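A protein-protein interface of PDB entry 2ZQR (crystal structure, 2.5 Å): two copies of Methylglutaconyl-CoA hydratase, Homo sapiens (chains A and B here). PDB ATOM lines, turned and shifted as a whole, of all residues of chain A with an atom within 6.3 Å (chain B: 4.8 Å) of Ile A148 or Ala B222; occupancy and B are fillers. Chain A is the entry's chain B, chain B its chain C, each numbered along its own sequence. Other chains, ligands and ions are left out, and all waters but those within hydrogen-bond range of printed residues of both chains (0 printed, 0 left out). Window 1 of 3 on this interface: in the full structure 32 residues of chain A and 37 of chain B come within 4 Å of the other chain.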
ATOM      1  N   VAL A  91     -17.742   3.609  -3.489  1.00  0.00           N
ATOM      2  CA  VAL A  91     -17.390   3.191  -2.144  1.00  0.00           C
ATOM      3  C   VAL A  91     -18.074   1.877  -1.805  1.00  0.00           C
ATOM      4  O   VAL A  91     -17.519   1.046  -1.080  1.00  0.00           O
ATOM      5  CB  VAL A  91     -17.784   4.254  -1.109  1.00  0.00           C
ATOM      6  CG1 VAL A  91     -17.559   3.719   0.293  1.00  0.00           C
ATOM      7  CG2 VAL A  91     -16.956   5.510  -1.323  1.00  0.00           C
ATOM      8  N   GLU A 122      -9.365  -1.568   6.673  1.00  0.00           N
ATOM      9  CA  GLU A 122     -10.625  -2.286   6.559  1.00  0.00           C
ATOM     10  C   GLU A 122     -10.418  -3.617   5.847  1.00  0.00           C
ATOM     11  O   GLU A 122     -11.094  -4.610   6.130  1.00  0.00           O
ATOM     12  CB  GLU A 122     -11.641  -1.414   5.823  1.00  0.00           C
ATOM     13  CG  GLU A 122     -11.749  -0.049   6.460  1.00  0.00           C
ATOM     14  CD  GLU A 122     -12.838   0.794   5.878  1.00  0.00           C
ATOM     15  OE1 GLU A 122     -13.935   0.828   6.474  1.00  0.00           O
ATOM     16  OE2 GLU A 122     -12.600   1.415   4.823  1.00  0.00           O
ATOM     17  N   GLU A 142     -11.096   8.881   8.297  1.00  0.00           N
ATOM     18  CA  GLU A 142     -12.142   9.427   7.431  1.00  0.00           C
ATOM     19  C   GLU A 142     -12.834  10.670   7.979  1.00  0.00           C
ATOM     20  O   GLU A 142     -13.160  11.579   7.218  1.00  0.00           O
ATOM     21  CB  GLU A 142     -13.212   8.366   7.139  1.00  0.00           C
ATOM     22  CG  GLU A 142     -12.872   7.370   6.033  1.00  0.00           C
ATOM     23  CD  GLU A 142     -11.821   6.355   6.442  1.00  0.00           C
ATOM     24  OE1 GLU A 142     -11.597   6.177   7.666  1.00  0.00           O
ATOM     25  OE2 GLU A 142     -11.234   5.726   5.532  1.00  0.00           O
ATOM     26  N   THR A 143     -13.072  10.707   9.286  1.00  0.00           N
ATOM     27  CA  THR A 143     -13.732  11.857   9.883  1.00  0.00           C
ATOM     28  C   THR A 143     -12.918  13.137   9.722  1.00  0.00           C
ATOM     29  O   THR A 143     -13.473  14.237   9.711  1.00  0.00           O
ATOM     30  CB  THR A 143     -14.027  11.623  11.369  1.00  0.00           C
ATOM     31  OG1 THR A 143     -12.830  11.218  12.035  1.00  0.00           O
ATOM     32  CG2 THR A 143     -15.091  10.547  11.531  1.00  0.00           C
ATOM     33  N   ALA A 146     -14.219  14.716   6.691  1.00  0.00           N
ATOM     34  CA  ALA A 146     -15.654  14.969   6.665  1.00  0.00           C
ATOM     35  C   ALA A 146     -16.517  13.773   6.213  1.00  0.00           C
ATOM     36  O   ALA A 146     -17.714  13.936   5.928  1.00  0.00           O
ATOM     37  CB  ALA A 146     -15.950  16.196   5.793  1.00  0.00           C
ATOM     38  N   ILE A 147     -15.923  12.580   6.150  1.00  0.00           N
ATOM     39  CA  ILE A 147     -16.680  11.380   5.766  1.00  0.00           C
ATOM     40  C   ILE A 147     -16.493  10.280   6.801  1.00  0.00           C
ATOM     41  O   ILE A 147     -16.032  10.544   7.910  1.00  0.00           O
ATOM     42  CB  ILE A 147     -16.234  10.842   4.418  1.00  0.00           C
ATOM     43  CG1 ILE A 147     -14.737  10.531   4.472  1.00  0.00           C
ATOM     44  CG2 ILE A 147     -16.572  11.845   3.343  1.00  0.00           C
ATOM     45  CD1 ILE A 147     -14.198   9.870   3.247  1.00  0.00           C
ATOM     46  N   ILE A 148     -16.851   9.051   6.447  1.00  0.00           N
ATOM     47  CA  ILE A 148     -16.697   7.927   7.373  1.00  0.00           C
ATOM     48  C   ILE A 148     -16.133   6.677   6.698  1.00  0.00           C
ATOM     49  O   ILE A 148     -16.081   6.591   5.469  1.00  0.00           O
ATOM     50  CB  ILE A 148     -18.045   7.538   8.021  1.00  0.00           C
ATOM     51  CG1 ILE A 148     -19.052   7.168   6.936  1.00  0.00           C
ATOM     52  CG2 ILE A 148     -18.557   8.678   8.876  1.00  0.00           C
ATOM     53  CD1 ILE A 148     -20.323   6.571   7.465  1.00  0.00           C
ATOM     54  N   PRO A 149     -15.684   5.694   7.499  1.00  0.00           N
ATOM     55  CA  PRO A 149     -15.145   4.469   6.899  1.00  0.00           C
ATOM     56  C   PRO A 149     -16.269   3.861   6.065  1.00  0.00           C
ATOM     57  O   PRO A 149     -17.402   3.749   6.532  1.00  0.00           O
ATOM     58  CB  PRO A 149     -14.803   3.612   8.110  1.00  0.00           C
ATOM     59  CG  PRO A 149     -14.449   4.645   9.162  1.00  0.00           C
ATOM     60  CD  PRO A 149     -15.509   5.695   8.963  1.00  0.00           C
ATOM     61  N   GLY A 150     -15.970   3.494   4.828  1.00  0.00           N
ATOM     62  CA  GLY A 150     -16.996   2.924   3.972  1.00  0.00           C
ATOM     63  C   GLY A 150     -16.588   1.587   3.395  1.00  0.00           C
ATOM     64  O   GLY A 150     -17.074   1.184   2.341  1.00  0.00           O
ATOM     65  N   GLY A 151     -15.678   0.910   4.090  1.00  0.00           N
ATOM     66  CA  GLY A 151     -15.211  -0.391   3.653  1.00  0.00           C
ATOM     67  C   GLY A 151     -15.516  -1.434   4.708  1.00  0.00           C
ATOM     68  O   GLY A 151     -14.895  -2.494   4.747  1.00  0.00           O
ATOM     69  N   THR A 154     -16.798   0.844  10.138  1.00  0.00           N
ATOM     70  CA  THR A 154     -17.699   1.167  11.235  1.00  0.00           C
ATOM     71  C   THR A 154     -18.290  -0.094  11.829  1.00  0.00           C
ATOM     72  O   THR A 154     -18.757  -0.090  12.963  1.00  0.00           O
ATOM     73  CB  THR A 154     -18.848   2.066  10.769  1.00  0.00           C
ATOM     74  OG1 THR A 154     -19.799   1.288  10.027  1.00  0.00           O
ATOM     75  CG2 THR A 154     -18.312   3.177   9.889  1.00  0.00           C
ATOM     76  N   ILE A 170     -12.265   6.401  15.648  1.00  0.00           N
ATOM     77  CA  ILE A 170     -12.967   7.012  14.520  1.00  0.00           C
ATOM     78  C   ILE A 170     -13.227   8.504  14.757  1.00  0.00           C
ATOM     79  O   ILE A 170     -13.093   9.322  13.844  1.00  0.00           O
ATOM     80  CB  ILE A 170     -14.335   6.343  14.260  1.00  0.00           C
ATOM     81  CG1 ILE A 170     -14.190   4.827  14.185  1.00  0.00           C
ATOM     82  CG2 ILE A 170     -14.911   6.856  12.956  1.00  0.00           C
ATOM     83  CD1 ILE A 170     -13.345   4.352  13.045  1.00  0.00           C
ATOM     84  N   PHE A 171     -13.620   8.840  15.983  1.00  0.00           N
ATOM     85  CA  PHE A 171     -13.918  10.217  16.353  1.00  0.00           C
ATOM     86  C   PHE A 171     -12.658  11.055  16.308  1.00  0.00           C
ATOM     87  O   PHE A 171     -12.697  12.212  15.889  1.00  0.00           O
ATOM     88  CB  PHE A 171     -14.487  10.297  17.773  1.00  0.00           C
ATOM     89  CG  PHE A 171     -15.838   9.657  17.948  1.00  0.00           C
ATOM     90  CD1 PHE A 171     -16.310   9.368  19.231  1.00  0.00           C
ATOM     91  CD2 PHE A 171     -16.642   9.349  16.854  1.00  0.00           C
ATOM     92  CE1 PHE A 171     -17.559   8.779  19.426  1.00  0.00           C
ATOM     93  CE2 PHE A 171     -17.905   8.756  17.034  1.00  0.00           C
ATOM     94  CZ  PHE A 171     -18.361   8.472  18.324  1.00  0.00           C
ATOM     95  N   ALA B 218     -20.192  14.032   9.595  1.00  0.00           N
ATOM     96  CA  ALA B 218     -19.535  12.750   9.493  1.00  0.00           C
ATOM     97  C   ALA B 218     -19.420  12.106  10.862  1.00  0.00           C
ATOM     98  O   ALA B 218     -19.518  10.891  10.988  1.00  0.00           O
ATOM     99  CB  ALA B 218     -18.160  12.920   8.879  1.00  0.00           C
ATOM    100  N   MET B 219     -19.228  12.921  11.890  1.00  0.00           N
ATOM    101  CA  MET B 219     -19.083  12.396  13.237  1.00  0.00           C
ATOM    102  C   MET B 219     -20.374  11.809  13.777  1.00  0.00           C
ATOM    103  O   MET B 219     -20.357  10.835  14.525  1.00  0.00           O
ATOM    104  CB  MET B 219     -18.593  13.493  14.182  1.00  0.00           C
ATOM    105  CG  MET B 219     -17.173  13.978  13.913  1.00  0.00           C
ATOM    106  SD  MET B 219     -15.882  12.849  14.527  1.00  0.00           S
ATOM    107  CE  MET B 219     -15.975  13.167  16.267  1.00  0.00           C
ATOM    108  N   ARG B 220     -21.498  12.400  13.398  1.00  0.00           N
ATOM    109  CA  ARG B 220     -22.785  11.918  13.884  1.00  0.00           C
ATOM    110  C   ARG B 220     -23.243  10.619  13.220  1.00  0.00           C
ATOM    111  O   ARG B 220     -23.697   9.698  13.903  1.00  0.00           O
ATOM    112  CB  ARG B 220     -23.852  13.017  13.735  1.00  0.00           C
ATOM    113  CG  ARG B 220     -23.522  14.263  14.551  1.00  0.00           C
ATOM    114  CD  ARG B 220     -24.708  15.199  14.702  1.00  0.00           C
ATOM    115  NE  ARG B 220     -24.351  16.423  15.419  1.00  0.00           N
ATOM    116  CZ  ARG B 220     -25.227  17.227  16.016  1.00  0.00           C
ATOM    117  NH1 ARG B 220     -26.521  16.936  15.988  1.00  0.00           N
ATOM    118  NH2 ARG B 220     -24.809  18.321  16.644  1.00  0.00           N
ATOM    119  N   VAL B 221     -23.125  10.539  11.896  1.00  0.00           N
ATOM    120  CA  VAL B 221     -23.532   9.328  11.195  1.00  0.00           C
ATOM    121  C   VAL B 221     -22.578   8.180  11.518  1.00  0.00           C
ATOM    122  O   VAL B 221     -22.944   7.006  11.418  1.00  0.00           O
ATOM    123  CB  VAL B 221     -23.628   9.546   9.653  1.00  0.00           C
ATOM    124  CG1 VAL B 221     -24.713  10.575   9.359  1.00  0.00           C
ATOM    125  CG2 VAL B 221     -22.283   9.977   9.065  1.00  0.00           C
ATOM    126  N   ALA B 222     -21.360   8.520  11.925  1.00  0.00           N
ATOM    127  CA  ALA B 222     -20.393   7.496  12.282  1.00  0.00           C
ATOM    128  C   ALA B 222     -20.862   6.878  13.591  1.00  0.00           C
ATOM    129  O   ALA B 222     -20.770   5.665  13.776  1.00  0.00           O
ATOM    130  CB  ALA B 222     -19.006   8.098  12.443  1.00  0.00           C
ATOM    131  N   LYS B 223     -21.387   7.704  14.493  1.00  0.00           N
ATOM    132  CA  LYS B 223     -21.870   7.182  15.767  1.00  0.00           C
ATOM    133  C   LYS B 223     -23.120   6.326  15.572  1.00  0.00           C
ATOM    134  O   LYS B 223     -23.310   5.329  16.273  1.00  0.00           O
ATOM    135  CB  LYS B 223     -22.165   8.305  16.765  1.00  0.00           C
ATOM    136  CG  LYS B 223     -22.701   7.769  18.094  1.00  0.00           C
ATOM    137  CD  LYS B 223     -22.775   8.823  19.177  1.00  0.00           C
ATOM    138  CE  LYS B 223     -23.101   8.170  20.507  1.00  0.00           C
ATOM    139  NZ  LYS B 223     -23.024   9.137  21.651  1.00  0.00           N
ATOM    140  N   LEU B 224     -23.962   6.726  14.617  1.00  0.00           N
ATOM    141  CA  LEU B 224     -25.181   5.997  14.293  1.00  0.00           C
ATOM    142  C   LEU B 224     -24.833   4.627  13.721  1.00  0.00           C
ATOM    143  O   LEU B 224     -25.380   3.600  14.149  1.00  0.00           O
ATOM    144  CB  LEU B 224     -26.009   6.762  13.256  1.00  0.00           C
ATOM    145  CG  LEU B 224     -26.736   8.013  13.731  1.00  0.00           C
ATOM    146  CD1 LEU B 224     -27.466   8.656  12.551  1.00  0.00           C
ATOM    147  CD2 LEU B 224     -27.711   7.652  14.854  1.00  0.00           C
ATOM    148  N   ALA B 225     -23.924   4.626  12.747  1.00  0.00           N
ATOM    149  CA  ALA B 225     -23.487   3.395  12.100  1.00  0.00           C
ATOM    150  C   ALA B 225     -22.977   2.402  13.137  1.00  0.00           C
ATOM    151  O   ALA B 225     -23.498   1.295  13.257  1.00  0.00           O
ATOM    152  CB  ALA B 225     -22.392   3.696  11.080  1.00  0.00           C
ATOM    153  N   ILE B 226     -21.966   2.816  13.895  1.00  0.00           N
ATOM    154  CA  ILE B 226     -21.367   1.956  14.910  1.00  0.00           C
ATOM    155  C   ILE B 226     -22.391   1.466  15.929  1.00  0.00           C
ATOM    156  O   ILE B 226     -22.575   0.262  16.098  1.00  0.00           O
ATOM    157  CB  ILE B 226     -20.210   2.690  15.639  1.00  0.00           C
ATOM    158  CG1 ILE B 226     -19.113   3.054  14.635  1.00  0.00           C
ATOM    159  CG2 ILE B 226     -19.634   1.811  16.733  1.00  0.00           C
ATOM    160  CD1 ILE B 226     -18.208   4.165  15.108  1.00  0.00           C
ATOM    161  N   GLU B 241     -23.986   1.246   7.397  1.00  0.00           N
ATOM    162  CA  GLU B 241     -22.791   2.055   7.170  1.00  0.00           C
ATOM    163  C   GLU B 241     -22.997   2.815   5.856  1.00  0.00           C
ATOM    164  O   GLU B 241     -22.792   4.024   5.786  1.00  0.00           O
ATOM    165  CB  GLU B 241     -21.539   1.168   7.076  1.00  0.00           C
ATOM    166  CG  GLU B 241     -20.248   1.928   6.724  1.00  0.00           C
ATOM    167  CD  GLU B 241     -19.008   1.031   6.703  1.00  0.00           C
ATOM    168  OE1 GLU B 241     -18.589   0.553   7.779  1.00  0.00           O
ATOM    169  OE2 GLU B 241     -18.450   0.807   5.610  1.00  0.00           O
ATOM    170  N   CYS B 244     -25.365   5.659   6.111  1.00  0.00           N
ATOM    171  CA  CYS B 244     -24.820   6.727   6.934  1.00  0.00           C
ATOM    172  C   CYS B 244     -23.802   7.501   6.100  1.00  0.00           C
ATOM    173  O   CYS B 244     -23.779   8.733   6.104  1.00  0.00           O
ATOM    174  CB  CYS B 244     -24.159   6.149   8.177  1.00  0.00           C
ATOM    175  SG  CYS B 244     -25.335   5.659   9.443  1.00  0.00           S
ATOM    176  N   TYR B 245     -22.976   6.766   5.367  1.00  0.00           N
ATOM    177  CA  TYR B 245     -21.959   7.366   4.511  1.00  0.00           C
ATOM    178  C   TYR B 245     -22.584   8.257   3.435  1.00  0.00           C
ATOM    179  O   TYR B 245     -22.101   9.358   3.175  1.00  0.00           O
ATOM    180  CB  TYR B 245     -21.129   6.273   3.830  1.00  0.00           C
ATOM    181  CG  TYR B 245     -19.982   6.820   3.019  1.00  0.00           C
ATOM    182  CD1 TYR B 245     -18.761   7.128   3.624  1.00  0.00           C
ATOM    183  CD2 TYR B 245     -20.121   7.059   1.655  1.00  0.00           C
ATOM    184  CE1 TYR B 245     -17.707   7.660   2.894  1.00  0.00           C
ATOM    185  CE2 TYR B 245     -19.072   7.596   0.910  1.00  0.00           C
ATOM    186  CZ  TYR B 245     -17.866   7.892   1.540  1.00  0.00           C
ATOM    187  OH  TYR B 245     -16.816   8.413   0.813  1.00  0.00           O
ATOM    188  N   THR B 248     -22.884  11.875   3.950  1.00  0.00           N
ATOM    189  CA  THR B 248     -21.731  12.768   3.962  1.00  0.00           C
ATOM    190  C   THR B 248     -21.365  13.148   2.536  1.00  0.00           C
ATOM    191  O   THR B 248     -20.627  14.112   2.303  1.00  0.00           O
ATOM    192  CB  THR B 248     -20.480  12.112   4.600  1.00  0.00           C
ATOM    193  OG1 THR B 248     -19.989  11.068   3.740  1.00  0.00           O
ATOM    194  CG2 THR B 248     -20.816  11.551   5.971  1.00  0.00           C
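Tyr B245 touches Val A91.
Ala A146 touches Ala B218.
Thr B248 touches Ala A146 (CB to O, 3.6 Å).
CG2 of Ile A147 touches OG1 of Thr B248, at 3.5 Å.
Ile A148 touches Ala B218.
CG2 of Ile A148 touches CB of Ala B222, at 3.6 Å.
CD1 of Ile A148 touches C of Cys B244, 3.9 Å away.
Gly A150 touches Glu B241 (C to OE2, 3.0 Å).
Ala B225 touches Thr A154 (CB to OG1, 3.7 Å).
Thr A154 touches Ile B226 (O to CG1, 3.6 Å).
Ile A148 touches just these residues of chain B: Ala B218, Val B221, Ala B222, Glu B241, Cys B244 and Tyr B245.
Of chain A, only Ile A148 comes within 4 Å of Ala B222.
Of the printed residues of chain A, Ala B225 touches Thr A154.
Printed residues of chain B within 4 Å of Phe A171: Met B219.
The nearest residue of chain A that does not touch Ala B222 is Ile A170 (4.3 Å).
The nearest printed residue of chain B that does not touch Thr A154 is Ala B222 (5.1 Å).
The side-chain carboxylate (OE2) of Glu B241 lies within hydrogen-bond range of the backbone NH (N) of Gly A151.
The side-chain hydroxyl (OG1) of Thr A154 sits at hydrogen-bond distance from the side-chain carboxylate (OE1) of Glu B241, 2.7 Å away.
The side-chain carboxylate (OE2) of Glu B241 lies close to the backbone carbonyl oxygen (O) of Pro A149.
O of Phe A171 sits close to SD of Met B219, at 3.5 Å.
No position is printed for both chains.
Of the 20 pairs that touch across the chains among the printed residues, none has its exchanged pair printed and touching as well.
The side-chain carboxylate (OE1) of Glu A122 is in hydrogen-bond range of the backbone NH (N) of Gly A151.
The backbone carbonyl oxygen (O) of Glu A142 is in hydrogen-bond range of the backbone NH (N) of Ile A147, at 3.1 Å.
The side-chain hydroxyl (OG1) of Thr A143 is in hydrogen-bond range of the backbone carbonyl oxygen (O) of Ile A170.
SG of Cys B244 is in hydrogen-bond range of O of Val B221 (3.4 Å).
The backbone NH (N) of Ala B225 is in hydrogen-bond range of the side-chain sulfur (SG) of Cys B244.
The side-chain hydroxyl of Thr B248 is in hydrogen-bond range of the backbone carbonyl oxygen of Tyr B245 (2.8 Å).
Of the 13 printed residues of chain A, 10 touch a printed residue of chain B.
Printed residues of chain A that touch a printed residue of chain B: Val A91, Thr A143, Ala A146, Ile A147, Ile A148, Pro A149, Gly A150, Gly A151, Thr A154 and Phe A171.
Among the printed residues, 20 pairs touch across the chains.
Among the printed residues, no Asp or Glu carboxylate lies within 4 Å of a Lys or Arg side-chain nitrogen of the other chain.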
